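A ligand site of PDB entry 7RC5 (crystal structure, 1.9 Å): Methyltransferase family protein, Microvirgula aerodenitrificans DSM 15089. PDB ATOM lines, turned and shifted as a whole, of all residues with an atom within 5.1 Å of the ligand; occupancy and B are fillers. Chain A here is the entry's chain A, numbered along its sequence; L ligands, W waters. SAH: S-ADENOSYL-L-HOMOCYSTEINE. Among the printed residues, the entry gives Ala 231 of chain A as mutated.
OD1 of Asp 185 lies within hydrogen-bond range of O2' of the ligand, 2.6 Å away.
OXT of the ligand is in hydrogen-bond range of OG of Ser 142.
The backbone carbonyl oxygen of Cys 164 is in hydrogen-bond range of a nitrogen (N) of the ligand (2.8 Å).
A nitrogen (N3) of the ligand sits at hydrogen-bond distance from the side-chain sulfur (SG) of Cys 164.
The backbone NH of Leu 215 lies within hydrogen-bond range of a nitrogen (N1) of the ligand.
The side-chain hydroxyl (OH) of Tyr 257 lies within hydrogen-bond range of a nitrogen (N6) of the ligand, 3.2 Å away.
N of Gly 166 sits at hydrogen-bond distance from OD2 of Asp 185, at 2.9 Å.
O of Asp 185 sits at hydrogen-bond distance from N of Glu 213.
The side-chain carboxylate (OD1) of Asp 185 lies within hydrogen-bond range of the backbone NH (N) of Gly 187 (2.9 Å).
O of Gly 139 sits at hydrogen-bond distance from OG of Ser 142.
The backbone NH of Cys 164 sits at hydrogen-bond distance from the backbone carbonyl oxygen of Thr 184, at 3.0 Å.
The backbone NH (N) of Thr 165 sits at hydrogen-bond distance from the backbone carbonyl oxygen (O) of Thr 184 (2.8 Å).
The side-chain hydroxyl (OG1) of Thr 165 lies within hydrogen-bond range of the side-chain carboxylate (OD2) of Asp 162, at 2.5 Å.
The backbone carbonyl oxygen (O) of Tyr 246 lies close to a sulfur (SD) of the ligand, at 3.7 Å.
Merely in contact with the ligand: Tyr 137, Ile 138, Thr 165, Gly 166, Ile 186, Pro 190, Glu 213, Asn 214, Ala 231, Pro 233 and Leu 245.
Hydrophobic or aromatic side chains within 4 Å of the ligand: Tyr 137, Ile 138, Ile 186, Pro 190, Leu 215, Ala 231, Pro 233, Leu 245, Tyr 246 and Tyr 257.
The nearest printed residue that does not touch the ligand is Ile 169 (4.02 Å).
Water W2 lies within hydrogen-bond range of the side-chain hydroxyl of Tyr 257 (2.5 Å) and a nitrogen (N7) of the ligand (2.8 Å).
Water W4 lies within hydrogen-bond range of the backbone carbonyl oxygen of Thr 165, the side-chain carboxylate of Asp 162, a nitrogen (N) of the ligand and the backbone NH of Ile 169.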
ATOM      1  N   TYR A 137      16.171  15.033   6.458  1.00  0.00           N
ATOM      2  CA  TYR A 137      14.841  14.650   5.996  1.00  0.00           C
ATOM      3  C   TYR A 137      14.328  13.437   6.780  1.00  0.00           C
ATOM      4  O   TYR A 137      15.097  12.563   7.187  1.00  0.00           O
ATOM      5  CB  TYR A 137      14.861  14.322   4.501  1.00  0.00           C
ATOM      6  CG  TYR A 137      13.520  13.839   3.987  1.00  0.00           C
ATOM      7  CD1 TYR A 137      12.534  14.750   3.666  1.00  0.00           C
ATOM      8  CD2 TYR A 137      13.229  12.480   3.886  1.00  0.00           C
ATOM      9  CE1 TYR A 137      11.302  14.333   3.219  1.00  0.00           C
ATOM     10  CE2 TYR A 137      11.994  12.049   3.441  1.00  0.00           C
ATOM     11  CZ  TYR A 137      11.024  12.985   3.115  1.00  0.00           C
ATOM     12  OH  TYR A 137       9.779  12.594   2.676  1.00  0.00           O
ATOM     13  N   ILE A 138      13.005  13.420   6.990  1.00  0.00           N
ATOM     14  CA  ILE A 138      12.251  12.190   7.256  1.00  0.00           C
ATOM     15  C   ILE A 138      10.835  12.401   6.725  1.00  0.00           C
ATOM     16  O   ILE A 138      10.284  13.494   6.843  1.00  0.00           O
ATOM     17  CB  ILE A 138      12.241  11.786   8.746  1.00  0.00           C
ATOM     18  CG1 ILE A 138      11.849  10.315   8.898  1.00  0.00           C
ATOM     19  CG2 ILE A 138      11.295  12.643   9.557  1.00  0.00           C
ATOM     20  CD1 ILE A 138      11.799   9.831  10.324  1.00  0.00           C
ATOM     21  N   GLY A 139      10.254  11.368   6.133  1.00  0.00           N
ATOM     22  CA  GLY A 139       8.915  11.505   5.610  1.00  0.00           C
ATOM     23  C   GLY A 139       8.125  10.212   5.672  1.00  0.00           C
ATOM     24  O   GLY A 139       8.635   9.176   6.134  1.00  0.00           O
ATOM     25  N   SER A 142       9.986   7.098   4.068  1.00  0.00           N
ATOM     26  CA  SER A 142      10.815   6.265   4.929  1.00  0.00           C
ATOM     27  C   SER A 142       9.978   5.191   5.620  1.00  0.00           C
ATOM     28  O   SER A 142      10.375   4.026   5.695  1.00  0.00           O
ATOM     29  CB  SER A 142      11.495   7.143   6.001  1.00  0.00           C
ATOM     30  OG  SER A 142      11.854   8.442   5.496  1.00  0.00           O
ATOM     31  N   ASP A 162      21.934   0.050   5.493  1.00  0.00           N
ATOM     32  CA  ASP A 162      21.009   1.150   5.208  1.00  0.00           C
ATOM     33  C   ASP A 162      21.834   2.284   4.614  1.00  0.00           C
ATOM     34  O   ASP A 162      22.586   2.952   5.332  1.00  0.00           O
ATOM     35  CB  ASP A 162      20.295   1.587   6.485  1.00  0.00           C
ATOM     36  CG  ASP A 162      19.379   2.773   6.256  1.00  0.00           C
ATOM     37  OD1 ASP A 162      18.681   2.800   5.210  1.00  0.00           O
ATOM     38  OD2 ASP A 162      19.360   3.688   7.118  1.00  0.00           O
ATOM     39  N   LEU A 163      21.683   2.507   3.307  1.00  0.00           N
ATOM     40  CA  LEU A 163      22.425   3.567   2.626  1.00  0.00           C
ATOM     41  C   LEU A 163      21.682   4.875   2.780  1.00  0.00           C
ATOM     42  O   LEU A 163      20.447   4.896   2.768  1.00  0.00           O
ATOM     43  CB  LEU A 163      22.568   3.233   1.131  1.00  0.00           C
ATOM     44  CG  LEU A 163      23.280   1.932   0.766  1.00  0.00           C
ATOM     45  CD1 LEU A 163      23.005   1.576  -0.710  1.00  0.00           C
ATOM     46  CD2 LEU A 163      24.763   2.099   1.011  1.00  0.00           C
ATOM     47  N   CYS A 164      22.433   5.986   2.879  1.00  0.00           N
ATOM     48  CA  CYS A 164      21.832   7.321   2.969  1.00  0.00           C
ATOM     49  C   CYS A 164      20.890   7.376   4.179  1.00  0.00           C
ATOM     50  O   CYS A 164      19.720   7.728   4.074  1.00  0.00           O
ATOM     51  CB  CYS A 164      21.098   7.703   1.679  1.00  0.00           C
ATOM     52  SG  CYS A 164      21.961   7.402   0.081  1.00  0.00           S
ATOM     53  N   THR A 165      21.443   7.022   5.332  1.00  0.00           N
ATOM     54  CA  THR A 165      20.624   6.708   6.497  1.00  0.00           C
ATOM     55  C   THR A 165      19.957   7.933   7.136  1.00  0.00           C
ATOM     56  O   THR A 165      18.934   7.781   7.810  1.00  0.00           O
ATOM     57  CB  THR A 165      21.486   5.960   7.503  1.00  0.00           C
ATOM     58  OG1 THR A 165      20.650   5.317   8.471  1.00  0.00           O
ATOM     59  CG2 THR A 165      22.444   6.926   8.221  1.00  0.00           C
ATOM     60  N   GLY A 166      20.496   9.132   6.940  1.00  0.00           N
ATOM     61  CA  GLY A 166      19.858  10.335   7.460  1.00  0.00           C
ATOM     62  C   GLY A 166      19.796  10.297   8.983  1.00  0.00           C
ATOM     63  O   GLY A 166      20.824  10.148   9.664  1.00  0.00           O
ATOM     64  N   SER A 167      18.587  10.409   9.528  1.00  0.00           N
ATOM     65  CA  SER A 167      18.403  10.301  10.978  1.00  0.00           C
ATOM     66  C   SER A 167      18.760   8.922  11.521  1.00  0.00           C
ATOM     67  O   SER A 167      19.018   8.785  12.721  1.00  0.00           O
ATOM     68  CB  SER A 167      16.951  10.646  11.343  1.00  0.00           C
ATOM     69  OG  SER A 167      16.049   9.640  10.850  1.00  0.00           O
ATOM     70  N   ILE A 169      16.719   6.038  10.897  1.00  0.00           N
ATOM     71  CA  ILE A 169      15.534   5.231  11.215  1.00  0.00           C
ATOM     72  C   ILE A 169      15.599   3.839  10.577  1.00  0.00           C
ATOM     73  O   ILE A 169      15.282   2.835  11.227  1.00  0.00           O
ATOM     74  CB  ILE A 169      14.248   5.979  10.819  1.00  0.00           C
ATOM     75  CG1 ILE A 169      13.028   5.139  11.161  1.00  0.00           C
ATOM     76  CG2 ILE A 169      14.239   6.350   9.328  1.00  0.00           C
ATOM     77  CD1 ILE A 169      11.754   5.778  10.679  1.00  0.00           C
ATOM     78  N   THR A 184      25.181   4.375   6.363  1.00  0.00           N
ATOM     79  CA  THR A 184      26.099   5.295   5.693  1.00  0.00           C
ATOM     80  C   THR A 184      25.427   6.630   5.398  1.00  0.00           C
ATOM     81  O   THR A 184      24.216   6.707   5.189  1.00  0.00           O
ATOM     82  CB  THR A 184      26.618   4.727   4.369  1.00  0.00           C
ATOM     83  OG1 THR A 184      25.543   4.732   3.407  1.00  0.00           O
ATOM     84  CG2 THR A 184      27.123   3.289   4.552  1.00  0.00           C
ATOM     85  N   ASP A 185      26.239   7.683   5.377  1.00  0.00           N
ATOM     86  CA  ASP A 185      25.775   8.987   4.925  1.00  0.00           C
ATOM     87  C   ASP A 185      27.028   9.804   4.630  1.00  0.00           C
ATOM     88  O   ASP A 185      28.143   9.371   4.912  1.00  0.00           O
ATOM     89  CB  ASP A 185      24.876   9.663   5.989  1.00  0.00           C
ATOM     90  CG  ASP A 185      23.881  10.633   5.383  1.00  0.00           C
ATOM     91  OD1 ASP A 185      24.303  11.677   4.819  1.00  0.00           O
ATOM     92  OD2 ASP A 185      22.656  10.373   5.469  1.00  0.00           O
ATOM     93  N   ILE A 186      26.849  10.974   4.018  1.00  0.00           N
ATOM     94  CA  ILE A 186      27.970  11.881   3.803  1.00  0.00           C
ATOM     95  C   ILE A 186      27.754  13.242   4.449  1.00  0.00           C
ATOM     96  O   ILE A 186      28.673  14.082   4.378  1.00  0.00           O
ATOM     97  CB  ILE A 186      28.298  12.054   2.307  1.00  0.00           C
ATOM     98  CG1 ILE A 186      27.064  12.554   1.564  1.00  0.00           C
ATOM     99  CG2 ILE A 186      28.736  10.717   1.713  1.00  0.00           C
ATOM    100  CD1 ILE A 186      27.327  12.934   0.139  1.00  0.00           C
ATOM    101  N   GLY A 187      26.600  13.509   5.042  1.00  0.00           N
ATOM    102  CA  GLY A 187      26.343  14.821   5.635  1.00  0.00           C
ATOM    103  C   GLY A 187      26.738  14.870   7.089  1.00  0.00           C
ATOM    104  O   GLY A 187      26.433  13.961   7.865  1.00  0.00           O
ATOM    105  N   PRO A 190      23.330  14.756   9.421  1.00  0.00           N
ATOM    106  CA  PRO A 190      22.735  13.428   9.653  1.00  0.00           C
ATOM    107  C   PRO A 190      23.699  12.459  10.322  1.00  0.00           C
ATOM    108  O   PRO A 190      23.269  11.700  11.200  1.00  0.00           O
ATOM    109  CB  PRO A 190      22.297  12.956   8.247  1.00  0.00           C
ATOM    110  CG  PRO A 190      23.053  13.792   7.275  1.00  0.00           C
ATOM    111  CD  PRO A 190      23.300  15.132   7.984  1.00  0.00           C
ATOM    112  N   GLU A 213      30.473   7.757   3.932  1.00  0.00           N
ATOM    113  CA  GLU A 213      30.861   7.122   2.667  1.00  0.00           C
ATOM    114  C   GLU A 213      29.808   7.378   1.598  1.00  0.00           C
ATOM    115  O   GLU A 213      28.605   7.231   1.849  1.00  0.00           O
ATOM    116  CB  GLU A 213      31.084   5.626   2.870  1.00  0.00           C
ATOM    117  CG  GLU A 213      31.533   4.886   1.626  1.00  0.00           C
ATOM    118  CD  GLU A 213      32.046   3.486   1.940  1.00  0.00           C
ATOM    119  OE1 GLU A 213      31.224   2.578   2.203  1.00  0.00           O
ATOM    120  OE2 GLU A 213      33.285   3.316   1.936  1.00  0.00           O
ATOM    121  N   ASN A 214      30.268   7.736   0.392  1.00  0.00           N
ATOM    122  CA  ASN A 214      29.371   7.943  -0.736  1.00  0.00           C
ATOM    123  C   ASN A 214      28.677   6.637  -1.101  1.00  0.00           C
ATOM    124  O   ASN A 214      29.270   5.565  -1.049  1.00  0.00           O
ATOM    125  CB  ASN A 214      30.146   8.431  -1.982  1.00  0.00           C
ATOM    126  CG  ASN A 214      30.863   9.755  -1.767  1.00  0.00           C
ATOM    127  OD1 ASN A 214      30.322  10.681  -1.195  1.00  0.00           O
ATOM    128  ND2 ASN A 214      32.073   9.850  -2.289  1.00  0.00           N
ATOM    129  N   LEU A 215      27.412   6.750  -1.513  1.00  0.00           N
ATOM    130  CA  LEU A 215      26.611   5.599  -1.939  1.00  0.00           C
ATOM    131  C   LEU A 215      27.366   4.710  -2.921  1.00  0.00           C
ATOM    132  O   LEU A 215      27.394   3.481  -2.781  1.00  0.00           O
ATOM    133  CB  LEU A 215      25.307   6.117  -2.555  1.00  0.00           C
ATOM    134  CG  LEU A 215      24.213   5.289  -3.218  1.00  0.00           C
ATOM    135  CD1 LEU A 215      22.952   6.106  -3.228  1.00  0.00           C
ATOM    136  CD2 LEU A 215      24.605   5.034  -4.643  1.00  0.00           C
ATOM    137  N   ALA A 231      16.428   4.933   1.032  1.00  0.00           N
ATOM    138  CA  ALA A 231      15.566   6.011   0.580  1.00  0.00           C
ATOM    139  C   ALA A 231      16.519   7.133   0.159  1.00  0.00           C
ATOM    140  O   ALA A 231      16.857   7.995   0.990  1.00  0.00           O
ATOM    141  CB  ALA A 231      14.625   6.477   1.693  1.00  0.00           C
ATOM    142  N   PRO A 232      16.996   7.154  -1.083  1.00  0.00           N
ATOM    143  CA  PRO A 232      18.060   8.104  -1.458  1.00  0.00           C
ATOM    144  C   PRO A 232      17.461   9.428  -1.873  1.00  0.00           C
ATOM    145  O   PRO A 232      16.238   9.506  -2.094  1.00  0.00           O
ATOM    146  CB  PRO A 232      18.737   7.409  -2.646  1.00  0.00           C
ATOM    147  CG  PRO A 232      17.570   6.738  -3.355  1.00  0.00           C
ATOM    148  CD  PRO A 232      16.568   6.341  -2.236  1.00  0.00           C
ATOM    149  N   PRO A 233      18.259  10.492  -2.001  1.00  0.00           N
ATOM    150  CA  PRO A 233      17.766  11.699  -2.683  1.00  0.00           C
ATOM    151  C   PRO A 233      17.211  11.316  -4.048  1.00  0.00           C
ATOM    152  O   PRO A 233      17.868  10.616  -4.821  1.00  0.00           O
ATOM    153  CB  PRO A 233      19.003  12.587  -2.794  1.00  0.00           C
ATOM    154  CG  PRO A 233      19.920  12.107  -1.715  1.00  0.00           C
ATOM    155  CD  PRO A 233      19.684  10.606  -1.647  1.00  0.00           C
ATOM    156  N   LEU A 245      21.293  18.674  -0.043  1.00  0.00           N
ATOM    157  CA  LEU A 245      21.947  17.369  -0.044  1.00  0.00           C
ATOM    158  C   LEU A 245      20.942  16.228   0.143  1.00  0.00           C
ATOM    159  O   LEU A 245      21.070  15.174  -0.480  1.00  0.00           O
ATOM    160  CB  LEU A 245      23.023  17.336   1.036  1.00  0.00           C
ATOM    161  CG  LEU A 245      23.846  16.073   1.188  1.00  0.00           C
ATOM    162  CD1 LEU A 245      24.723  15.803  -0.040  1.00  0.00           C
ATOM    163  CD2 LEU A 245      24.700  16.220   2.428  1.00  0.00           C
ATOM    164  N   TYR A 246      19.924  16.424   0.978  1.00  0.00           N
ATOM    165  CA  TYR A 246      19.043  15.293   1.279  1.00  0.00           C
ATOM    166  C   TYR A 246      17.919  15.127   0.269  1.00  0.00           C
ATOM    167  O   TYR A 246      17.294  14.063   0.237  1.00  0.00           O
ATOM    168  CB  TYR A 246      18.439  15.423   2.673  1.00  0.00           C
ATOM    169  CG  TYR A 246      17.671  16.703   2.907  1.00  0.00           C
ATOM    170  CD1 TYR A 246      16.374  16.858   2.425  1.00  0.00           C
ATOM    171  CD2 TYR A 246      18.270  17.770   3.564  1.00  0.00           C
ATOM    172  CE1 TYR A 246      15.671  18.040   2.633  1.00  0.00           C
ATOM    173  CE2 TYR A 246      17.587  18.954   3.762  1.00  0.00           C
ATOM    174  CZ  TYR A 246      16.289  19.090   3.304  1.00  0.00           C
ATOM    175  OH  TYR A 246      15.630  20.272   3.526  1.00  0.00           O
ATOM    176  N   TYR A 257      20.613   7.993  -8.507  1.00  0.00           N
ATOM    177  CA  TYR A 257      20.951   7.144  -7.369  1.00  0.00           C
ATOM    178  C   TYR A 257      20.132   5.856  -7.367  1.00  0.00           C
ATOM    179  O   TYR A 257      20.634   4.810  -6.940  1.00  0.00           O
ATOM    180  CB  TYR A 257      20.714   7.904  -6.063  1.00  0.00           C
ATOM    181  CG  TYR A 257      21.763   8.930  -5.728  1.00  0.00           C
ATOM    182  CD1 TYR A 257      23.100   8.756  -6.088  1.00  0.00           C
ATOM    183  CD2 TYR A 257      21.410  10.122  -5.092  1.00  0.00           C
ATOM    184  CE1 TYR A 257      24.071   9.732  -5.770  1.00  0.00           C
ATOM    185  CE2 TYR A 257      22.382  11.104  -4.782  1.00  0.00           C
ATOM    186  CZ  TYR A 257      23.696  10.902  -5.114  1.00  0.00           C
ATOM    187  OH  TYR A 257      24.645  11.869  -4.791  1.00  0.00           O
HETATM  188  N   SAH L   1      17.071   7.361   4.728  1.00  0.00           N
HETATM  189  CA  SAH L   1      16.546   8.442   5.564  1.00  0.00           C
HETATM  190  CB  SAH L   1      17.065   9.789   5.076  1.00  0.00           C
HETATM  191  CG  SAH L   1      17.007   9.928   3.566  1.00  0.00           C
HETATM  192  SD  SAH L   1      17.272  11.645   3.081  1.00  0.00           S
HETATM  193  C   SAH L   1      15.023   8.414   5.580  1.00  0.00           C
HETATM  194  O   SAH L   1      14.387   9.093   6.387  1.00  0.00           O
HETATM  195  OXT SAH L   1      14.393   7.700   4.779  1.00  0.00           O
HETATM  196  C5' SAH L   1      18.685  11.207   2.018  1.00  0.00           C
HETATM  197  C4' SAH L   1      20.032  11.140   2.750  1.00  0.00           C
HETATM  198  O4' SAH L   1      21.051  10.835   1.817  1.00  0.00           O
HETATM  199  C3' SAH L   1      20.491  12.448   3.402  1.00  0.00           C
HETATM  200  O3' SAH L   1      20.769  12.198   4.769  1.00  0.00           O
HETATM  201  C2' SAH L   1      21.784  12.842   2.686  1.00  0.00           C
HETATM  202  O2' SAH L   1      22.793  13.326   3.534  1.00  0.00           O
HETATM  203  C1' SAH L   1      22.267  11.512   2.162  1.00  0.00           C
HETATM  204  N9  SAH L   1      23.075  11.521   0.934  1.00  0.00           N
HETATM  205  C8  SAH L   1      22.972  12.362  -0.151  1.00  0.00           C
HETATM  206  N7  SAH L   1      23.872  11.952  -1.082  1.00  0.00           N
HETATM  207  C5  SAH L   1      24.520  10.841  -0.624  1.00  0.00           C
HETATM  208  C6  SAH L   1      25.506  10.007  -1.148  1.00  0.00           C
HETATM  209  N6  SAH L   1      26.039  10.208  -2.373  1.00  0.00           N
HETATM  210  N1  SAH L   1      25.957   8.959  -0.379  1.00  0.00           N
HETATM  211  C2  SAH L   1      25.434   8.701   0.865  1.00  0.00           C
HETATM  212  N3  SAH L   1      24.464   9.529   1.372  1.00  0.00           N
HETATM  213  C4  SAH L   1      24.009  10.575   0.640  1.00  0.00           C
HETATM  214  O   HOH W   1      21.028  15.785   4.498  1.00  0.00           O
HETATM  215  O   HOH W   2      24.039  13.763  -3.202  1.00  0.00           O
HETATM  216  O   HOH W   3      17.884   4.952   3.720  1.00  0.00           O
HETATM  217  O   HOH W   4      17.307   5.604   7.478  1.00  0.00           O
